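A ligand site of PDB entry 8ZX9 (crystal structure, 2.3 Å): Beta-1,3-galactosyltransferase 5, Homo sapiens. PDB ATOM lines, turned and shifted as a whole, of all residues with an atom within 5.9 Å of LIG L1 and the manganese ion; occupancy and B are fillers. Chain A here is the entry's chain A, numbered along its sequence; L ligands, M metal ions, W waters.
O2 of LG2 L2 lies within hydrogen-bond range of OD2 of Asp 126, at 2.5 Å. An oxygen (O5) of LIG L1 is in hydrogen-bond range of the backbone NH (N) of Ser 127 (3.1 Å). The backbone carbonyl oxygen (O) of Thr 34 sits at hydrogen-bond distance from an oxygen (O5) of LIG L1 (2.9 Å). The side-chain amino group (NZ) of Lys 167 is in salt-bridge range of an oxygen (O11) of LIG L1 (2.9 Å). O3 of LIG L1 lies within hydrogen-bond range of OE1 of Gln 39, 2.7 Å away. N of Ser 35 lies close to O1 of LIG L1. O4 of LG2 L2 lies within hydrogen-bond range of OH of Tyr 98 (3.4 Å). NZ of Lys 104 sits at hydrogen-bond distance from O1 of LIG L1. OH of Tyr 98 lies within hydrogen-bond range of O10 of LIG L1 (2.8 Å). OG of Ser 127 sits at hydrogen-bond distance from O3 of LIG L1, at 3.0 Å. The side-chain hydroxyl (OG1) of Thr 34 lies within hydrogen-bond range of an oxygen (O5) of LIG L1 (2.8 Å). The side-chain carboxylate (OD1) of Asp 96 is in hydrogen-bond range of a nitrogen (N2) of LIG L1 (2.9 Å).
O1 of LG2 L2 sits at hydrogen-bond distance from O10 of LIG L1, at 3.2 Å.
OD2 of Asp 96 lies within salt-bridge range of NZ of Lys 104 (2.8 Å). The backbone carbonyl oxygen (O) of Thr 187 sits at hydrogen-bond distance from the backbone NH (N) of Asp 126, 3.1 Å away. O of Asp 128 is in hydrogen-bond range of N of Phe 256 (3.2 Å). The backbone carbonyl oxygen (O) of Thr 34 sits close to the side-chain hydroxyl (OG) of Ser 127 (3.3 Å). The side-chain hydroxyl of Tyr 98 sits at hydrogen-bond distance from the indole nitrogen of Trp 168 (2.7 Å). The side-chain amide oxygen of Gln 39 lies within hydrogen-bond range of the backbone NH of Ser 36, at 2.9 Å. The side-chain amino group (NZ) of Lys 104 lies within hydrogen-bond range of the backbone carbonyl oxygen (O) of Leu 66 (3.0 Å). O of Thr 125 sits at hydrogen-bond distance from N of Thr 34 (3.0 Å).
Ser 36 touches LIG L1. Val 97 touches LIG L1 (CA to O2, 3.2 Å). Leu 101 touches LIG L1 (CD1 to O4, 3.4 Å). Asp 126 touches LIG L1. Trp 168 touches LIG L1 (CZ2 to O11, 3.4 Å). 15 residues have an atom within 4 Å of LIG L1: Thr 34, Ser 35, Ser 36, Gln 39, Asp 96, Val 97, Tyr 98, Leu 101, Lys 104, Asp 126, Ser 127, Asp 128, Lys 167, Trp 168 and His 255.
Of the 20 residues printed, 2 come within 4 Å of the manganese ion. The nearest printed residue that does not touch the manganese ion is Asp 126 (4.8 Å).
The manganese ion is bound by O12 of LIG L1 (1.8 Å), OD2 of Asp 128 (2.0 Å), NE2 of His 255 (2.2 Å), water W1 (2.3 Å), O8 of LIG L1 (2.4 Å) and water W2 (2.7 Å). The manganese ion has six donor atoms within binding distance.
Water W1 lies within hydrogen-bond range of the side-chain carboxylate (OD1) of Asp 128 (2.6 Å) and the side-chain carboxylate (OD2) of Asp 126 (2.7 Å).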
ATOM      1  N   THR A  34      -3.663  16.273   5.161  1.00  0.00           N
ATOM      2  CA  THR A  34      -2.567  16.520   6.101  1.00  0.00           C
ATOM      3  C   THR A  34      -2.625  17.951   6.618  1.00  0.00           C
ATOM      4  O   THR A  34      -2.753  18.872   5.802  1.00  0.00           O
ATOM      5  CB  THR A  34      -1.257  16.234   5.386  1.00  0.00           C
ATOM      6  OG1 THR A  34      -1.068  17.259   4.414  1.00  0.00           O
ATOM      7  CG2 THR A  34      -1.275  14.866   4.732  1.00  0.00           C
ATOM      8  N   SER A  35      -2.558  18.120   7.936  1.00  0.00           N
ATOM      9  CA  SER A  35      -2.512  19.457   8.561  1.00  0.00           C
ATOM     10  C   SER A  35      -1.859  19.298   9.934  1.00  0.00           C
ATOM     11  O   SER A  35      -2.115  18.285  10.569  1.00  0.00           O
ATOM     12  CB  SER A  35      -3.868  20.102   8.655  1.00  0.00           C
ATOM     13  OG  SER A  35      -4.701  19.402   9.568  1.00  0.00           O
ATOM     14  N   SER A  36      -1.038  20.251  10.363  1.00  0.00           N
ATOM     15  CA  SER A  36      -0.512  20.188  11.716  1.00  0.00           C
ATOM     16  C   SER A  36      -1.578  20.645  12.710  1.00  0.00           C
ATOM     17  O   SER A  36      -2.626  21.162  12.347  1.00  0.00           O
ATOM     18  CB  SER A  36       0.753  21.033  11.834  1.00  0.00           C
ATOM     19  OG  SER A  36       0.511  22.381  11.522  1.00  0.00           O
ATOM     20  N   HIS A  37      -1.273  20.459  13.999  1.00  0.00           N
ATOM     21  CA  HIS A  37      -2.267  20.693  15.054  1.00  0.00           C
ATOM     22  C   HIS A  37      -2.786  22.131  15.050  1.00  0.00           C
ATOM     23  O   HIS A  37      -3.995  22.366  15.179  1.00  0.00           O
ATOM     24  CB  HIS A  37      -1.660  20.364  16.411  1.00  0.00           C
ATOM     25  CG  HIS A  37      -1.426  18.905  16.621  1.00  0.00           C
ATOM     26  ND1 HIS A  37      -2.245  18.132  17.414  1.00  0.00           N
ATOM     27  CD2 HIS A  37      -0.487  18.066  16.109  1.00  0.00           C
ATOM     28  CE1 HIS A  37      -1.814  16.889  17.406  1.00  0.00           C
ATOM     29  NE2 HIS A  37      -0.751  16.825  16.617  1.00  0.00           N
ATOM     30  N   GLN A  39      -3.146  24.189  12.773  1.00  0.00           N
ATOM     31  CA  GLN A  39      -3.827  24.619  11.528  1.00  0.00           C
ATOM     32  C   GLN A  39      -5.334  24.330  11.605  1.00  0.00           C
ATOM     33  O   GLN A  39      -5.873  23.768  10.652  1.00  0.00           O
ATOM     34  CB  GLN A  39      -3.152  23.978  10.313  1.00  0.00           C
ATOM     35  CG  GLN A  39      -1.812  24.595   9.937  1.00  0.00           C
ATOM     36  CD  GLN A  39      -1.160  23.892   8.773  1.00  0.00           C
ATOM     37  OE1 GLN A  39      -0.837  22.711   8.832  1.00  0.00           O
ATOM     38  NE2 GLN A  39      -0.960  24.629   7.678  1.00  0.00           N
ATOM     39  N   LEU A  66      -5.717  13.785   8.862  1.00  0.00           N
ATOM     40  CA  LEU A  66      -4.643  13.007   9.456  1.00  0.00           C
ATOM     41  C   LEU A  66      -3.858  13.873  10.435  1.00  0.00           C
ATOM     42  O   LEU A  66      -3.385  14.953  10.076  1.00  0.00           O
ATOM     43  CB  LEU A  66      -3.719  12.485   8.362  1.00  0.00           C
ATOM     44  CG  LEU A  66      -4.320  11.812   7.107  1.00  0.00           C
ATOM     45  CD1 LEU A  66      -3.264  11.323   6.090  1.00  0.00           C
ATOM     46  CD2 LEU A  66      -5.260  10.665   7.464  1.00  0.00           C
ATOM     47  N   ASP A  96       4.039  14.861  15.230  1.00  0.00           N
ATOM     48  CA  ASP A  96       3.561  15.528  13.999  1.00  0.00           C
ATOM     49  C   ASP A  96       4.497  16.678  13.617  1.00  0.00           C
ATOM     50  O   ASP A  96       4.282  17.791  14.082  1.00  0.00           O
ATOM     51  CB  ASP A  96       2.109  15.950  14.125  1.00  0.00           C
ATOM     52  CG  ASP A  96       1.361  16.226  12.831  1.00  0.00           C
ATOM     53  OD1 ASP A  96       2.031  16.302  11.781  1.00  0.00           O
ATOM     54  OD2 ASP A  96       0.124  16.362  12.891  1.00  0.00           O
ATOM     55  N   VAL A  97       5.508  16.371  12.805  1.00  0.00           N
ATOM     56  CA  VAL A  97       6.471  17.384  12.294  1.00  0.00           C
ATOM     57  C   VAL A  97       6.645  17.131  10.783  1.00  0.00           C
ATOM     58  O   VAL A  97       6.293  16.036  10.331  1.00  0.00           O
ATOM     59  CB  VAL A  97       7.800  17.258  13.063  1.00  0.00           C
ATOM     60  CG1 VAL A  97       7.694  17.754  14.495  1.00  0.00           C
ATOM     61  CG2 VAL A  97       8.372  15.850  13.010  1.00  0.00           C
ATOM     62  N   TYR A  98       7.181  18.101  10.045  1.00  0.00           N
ATOM     63  CA  TYR A  98       7.388  17.976   8.580  1.00  0.00           C
ATOM     64  C   TYR A  98       8.179  16.706   8.239  1.00  0.00           C
ATOM     65  O   TYR A  98       7.822  16.071   7.230  1.00  0.00           O
ATOM     66  CB  TYR A  98       8.039  19.226   7.989  1.00  0.00           C
ATOM     67  CG  TYR A  98       7.943  19.327   6.470  1.00  0.00           C
ATOM     68  CD1 TYR A  98       6.821  19.890   5.863  1.00  0.00           C
ATOM     69  CD2 TYR A  98       8.956  18.862   5.651  1.00  0.00           C
ATOM     70  CE1 TYR A  98       6.724  19.974   4.488  1.00  0.00           C
ATOM     71  CE2 TYR A  98       8.867  18.936   4.270  1.00  0.00           C
ATOM     72  CZ  TYR A  98       7.746  19.498   3.696  1.00  0.00           C
ATOM     73  OH  TYR A  98       7.653  19.587   2.334  1.00  0.00           O
ATOM     74  N   LEU A 101       6.089  13.265   7.934  1.00  0.00           N
ATOM     75  CA  LEU A 101       4.942  13.207   6.988  1.00  0.00           C
ATOM     76  C   LEU A 101       4.832  11.811   6.329  1.00  0.00           C
ATOM     77  O   LEU A 101       3.728  11.427   5.967  1.00  0.00           O
ATOM     78  CB  LEU A 101       5.105  14.347   5.984  1.00  0.00           C
ATOM     79  CG  LEU A 101       4.624  15.722   6.463  1.00  0.00           C
ATOM     80  CD1 LEU A 101       4.916  16.784   5.423  1.00  0.00           C
ATOM     81  CD2 LEU A 101       3.151  15.703   6.816  1.00  0.00           C
ATOM     82  N   LYS A 104       2.697  10.029   8.684  1.00  0.00           N
ATOM     83  CA  LYS A 104       1.306  10.515   8.502  1.00  0.00           C
ATOM     84  C   LYS A 104       0.717   9.847   7.241  1.00  0.00           C
ATOM     85  O   LYS A 104      -0.401   9.336   7.333  1.00  0.00           O
ATOM     86  CB  LYS A 104       1.210  12.035   8.381  1.00  0.00           C
ATOM     87  CG  LYS A 104      -0.194  12.597   8.374  1.00  0.00           C
ATOM     88  CD  LYS A 104      -0.212  14.102   8.562  1.00  0.00           C
ATOM     89  CE  LYS A 104       0.051  14.490   9.968  1.00  0.00           C
ATOM     90  NZ  LYS A 104      -0.486  15.820  10.251  1.00  0.00           N
ATOM     91  N   THR A 125      -4.189  14.621   0.203  1.00  0.00           N
ATOM     92  CA  THR A 125      -3.972  16.021  -0.187  1.00  0.00           C
ATOM     93  C   THR A 125      -3.429  16.817   0.955  1.00  0.00           C
ATOM     94  O   THR A 125      -3.564  16.419   2.125  1.00  0.00           O
ATOM     95  CB  THR A 125      -5.263  16.667  -0.722  1.00  0.00           C
ATOM     96  OG1 THR A 125      -4.871  17.946  -1.211  1.00  0.00           O
ATOM     97  CG2 THR A 125      -6.325  16.819   0.344  1.00  0.00           C
ATOM     98  N   ASP A 126      -2.853  17.944   0.604  1.00  0.00           N
ATOM     99  CA  ASP A 126      -2.376  18.873   1.640  1.00  0.00           C
ATOM    100  C   ASP A 126      -3.483  19.875   1.987  1.00  0.00           C
ATOM    101  O   ASP A 126      -4.546  19.837   1.350  1.00  0.00           O
ATOM    102  CB  ASP A 126      -1.020  19.369   1.205  1.00  0.00           C
ATOM    103  CG  ASP A 126       0.074  18.312   1.208  1.00  0.00           C
ATOM    104  OD1 ASP A 126      -0.070  17.323   1.955  1.00  0.00           O
ATOM    105  OD2 ASP A 126       1.059  18.488   0.474  1.00  0.00           O
ATOM    106  N   SER A 127      -3.224  20.755   2.943  1.00  0.00           N
ATOM    107  CA  SER A 127      -4.254  21.683   3.473  1.00  0.00           C
ATOM    108  C   SER A 127      -4.195  23.071   2.796  1.00  0.00           C
ATOM    109  O   SER A 127      -5.151  23.817   2.957  1.00  0.00           O
ATOM    110  CB  SER A 127      -4.082  21.776   4.964  1.00  0.00           C
ATOM    111  OG  SER A 127      -2.769  22.157   5.319  1.00  0.00           O
ATOM    112  N   ASP A 128      -3.116  23.370   2.081  1.00  0.00           N
ATOM    113  CA  ASP A 128      -2.917  24.661   1.364  1.00  0.00           C
ATOM    114  C   ASP A 128      -3.395  24.451  -0.075  1.00  0.00           C
ATOM    115  O   ASP A 128      -2.667  24.799  -1.003  1.00  0.00           O
ATOM    116  CB  ASP A 128      -1.469  25.095   1.456  1.00  0.00           C
ATOM    117  CG  ASP A 128      -0.439  24.020   1.126  1.00  0.00           C
ATOM    118  OD1 ASP A 128      -0.823  22.848   1.017  1.00  0.00           O
ATOM    119  OD2 ASP A 128       0.739  24.372   0.976  1.00  0.00           O
ATOM    120  N   LYS A 167      14.750  22.904   2.499  1.00  0.00           N
ATOM    121  CA  LYS A 167      13.708  22.186   3.267  1.00  0.00           C
ATOM    122  C   LYS A 167      13.659  20.729   2.782  1.00  0.00           C
ATOM    123  O   LYS A 167      13.388  19.846   3.585  1.00  0.00           O
ATOM    124  CB  LYS A 167      12.377  22.910   3.036  1.00  0.00           C
ATOM    125  CG  LYS A 167      11.151  22.354   3.742  1.00  0.00           C
ATOM    126  CD  LYS A 167       9.908  23.166   3.411  1.00  0.00           C
ATOM    127  CE  LYS A 167       8.754  22.896   4.309  1.00  0.00           C
ATOM    128  NZ  LYS A 167       7.509  23.436   3.771  1.00  0.00           N
ATOM    129  N   TRP A 168      13.951  20.521   1.494  1.00  0.00           N
ATOM    130  CA  TRP A 168      13.798  19.135   1.023  1.00  0.00           C
ATOM    131  C   TRP A 168      15.148  18.448   0.788  1.00  0.00           C
ATOM    132  O   TRP A 168      15.183  17.504  -0.001  1.00  0.00           O
ATOM    133  CB  TRP A 168      12.921  19.154  -0.228  1.00  0.00           C
ATOM    134  CG  TRP A 168      11.647  19.928   0.000  1.00  0.00           C
ATOM    135  CD1 TRP A 168      10.523  19.484   0.631  1.00  0.00           C
ATOM    136  CD2 TRP A 168      11.397  21.289  -0.372  1.00  0.00           C
ATOM    137  NE1 TRP A 168       9.590  20.484   0.660  1.00  0.00           N
ATOM    138  CE2 TRP A 168      10.090  21.599   0.058  1.00  0.00           C
ATOM    139  CE3 TRP A 168      12.151  22.277  -1.016  1.00  0.00           C
ATOM    140  CZ2 TRP A 168       9.519  22.849  -0.138  1.00  0.00           C
ATOM    141  CZ3 TRP A 168      11.583  23.518  -1.209  1.00  0.00           C
ATOM    142  CH2 TRP A 168      10.288  23.801  -0.772  1.00  0.00           C
ATOM    143  N   THR A 187       1.308  17.240  -2.966  1.00  0.00           N
ATOM    144  CA  THR A 187       0.263  18.275  -2.879  1.00  0.00           C
ATOM    145  C   THR A 187      -1.090  17.618  -3.031  1.00  0.00           C
ATOM    146  O   THR A 187      -2.052  18.085  -2.409  1.00  0.00           O
ATOM    147  CB  THR A 187       0.487  19.311  -3.989  1.00  0.00           C
ATOM    148  OG1 THR A 187       0.488  18.669  -5.258  1.00  0.00           O
ATOM    149  CG2 THR A 187       1.767  20.100  -3.772  1.00  0.00           C
ATOM    150  N   HIS A 255      -2.381  24.236  -5.724  1.00  0.00           N
ATOM    151  CA  HIS A 255      -1.601  24.498  -4.485  1.00  0.00           C
ATOM    152  C   HIS A 255      -1.402  26.000  -4.235  1.00  0.00           C
ATOM    153  O   HIS A 255      -1.807  26.792  -5.085  1.00  0.00           O
ATOM    154  CB  HIS A 255      -0.291  23.696  -4.586  1.00  0.00           C
ATOM    155  CG  HIS A 255       0.606  23.653  -3.411  1.00  0.00           C
ATOM    156  ND1 HIS A 255       1.942  23.958  -3.532  1.00  0.00           N
ATOM    157  CD2 HIS A 255       0.428  23.324  -2.135  1.00  0.00           C
ATOM    158  CE1 HIS A 255       2.530  23.839  -2.355  1.00  0.00           C
ATOM    159  NE2 HIS A 255       1.621  23.452  -1.492  1.00  0.00           N
ATOM    160  N   PHE A 256      -0.811  26.354  -3.098  1.00  0.00           N
ATOM    161  CA  PHE A 256      -0.528  27.766  -2.693  1.00  0.00           C
ATOM    162  C   PHE A 256      -1.831  28.493  -2.386  1.00  0.00           C
ATOM    163  O   PHE A 256      -2.024  29.589  -2.874  1.00  0.00           O
ATOM    164  CB  PHE A 256       0.386  28.461  -3.713  1.00  0.00           C
ATOM    165  CG  PHE A 256       1.749  27.804  -3.901  1.00  0.00           C
ATOM    166  CD1 PHE A 256       2.643  27.694  -2.843  1.00  0.00           C
ATOM    167  CD2 PHE A 256       2.138  27.313  -5.144  1.00  0.00           C
ATOM    168  CE1 PHE A 256       3.881  27.109  -3.026  1.00  0.00           C
ATOM    169  CE2 PHE A 256       3.377  26.742  -5.318  1.00  0.00           C
ATOM    170  CZ  PHE A 256       4.246  26.633  -4.259  1.00  0.00           C
HETATM  171  N1  LIG L   1       2.060  19.305   7.729  1.00  0.00           N
HETATM  172  C1  LIG L   1       1.632  18.441   8.724  1.00  0.00           C
HETATM  173  N2  LIG L   1       2.376  18.481   9.868  1.00  0.00           N
HETATM  174  C2  LIG L   1       3.476  19.269  10.116  1.00  0.00           C
HETATM  175  C3  LIG L   1       3.847  20.142   9.040  1.00  0.00           C
HETATM  176  C4  LIG L   1       3.141  20.133   7.910  1.00  0.00           C
HETATM  177  O1  LIG L   1       0.680  17.693   8.592  1.00  0.00           O
HETATM  178  O2  LIG L   1       4.033  19.204  11.209  1.00  0.00           O
HETATM  179  C5  LIG L   1       1.297  19.315   6.474  1.00  0.00           C
HETATM  180  C6  LIG L   1       0.904  20.721   6.036  1.00  0.00           C
HETATM  181  O3  LIG L   1      -0.296  21.118   6.658  1.00  0.00           O
HETATM  182  C7  LIG L   1       0.745  20.505   4.528  1.00  0.00           C
HETATM  183  C8  LIG L   1       1.855  19.500   4.205  1.00  0.00           C
HETATM  184  O4  LIG L   1       2.136  18.809   5.451  1.00  0.00           O
HETATM  185  O5  LIG L   1      -0.544  19.977   4.251  1.00  0.00           O
HETATM  186  C9  LIG L   1       3.143  20.065   3.635  1.00  0.00           C
HETATM  187  O6  LIG L   1       3.576  21.210   4.424  1.00  0.00           O
HETATM  188  P1  LIG L   1       3.832  22.616   3.711  1.00  0.00           P
HETATM  189  O7  LIG L   1       4.322  23.595   4.705  1.00  0.00           O
HETATM  190  O8  LIG L   1       2.620  22.980   2.930  1.00  0.00           O
HETATM  191  O9  LIG L   1       5.047  22.241   2.743  1.00  0.00           O
HETATM  192  P2  LIG L   1       5.360  22.393   1.180  1.00  0.00           P
HETATM  193  O10 LIG L   1       5.830  21.050   0.749  1.00  0.00           O
HETATM  194  O11 LIG L   1       6.425  23.422   1.096  1.00  0.00           O
HETATM  195  O12 LIG L   1       4.061  22.810   0.520  1.00  0.00           O
HETATM  196  C1  LG2 L   2       6.229  17.931  -0.839  1.00  0.00           C
HETATM  197  C2  LG2 L   2       4.729  17.738  -0.668  1.00  0.00           C
HETATM  198  C3  LG2 L   2       4.363  17.228   0.695  1.00  0.00           C
HETATM  199  C4  LG2 L   2       5.163  15.973   0.926  1.00  0.00           C
HETATM  200  C5  LG2 L   2       6.630  16.383   1.062  1.00  0.00           C
HETATM  201  C6  LG2 L   2       7.551  15.202   1.251  1.00  0.00           C
HETATM  202  O1  LG2 L   2       4.046  18.955  -0.932  1.00  0.00           O
HETATM  203  O2  LG2 L   2       2.979  16.955   0.803  1.00  0.00           O
HETATM  204  O3  LG2 L   2       4.984  15.059  -0.156  1.00  0.00           O
HETATM  205  O4  LG2 L   2       7.146  17.178  -0.031  1.00  0.00           O
HETATM  206  O5  LG2 L   2       7.565  14.824   2.627  1.00  0.00           O
HETATM  207 MN    MN M   1       2.290  23.105   0.562  1.00  0.00          MN
HETATM  208  O   HOH W   1       1.088  21.173   0.272  1.00  0.00           O
HETATM  209  O   HOH W   2       3.605  25.404   0.825  1.00  0.00           O
HETATM  210  O   HOH W   3       3.237  23.829   6.915  1.00  0.00           O
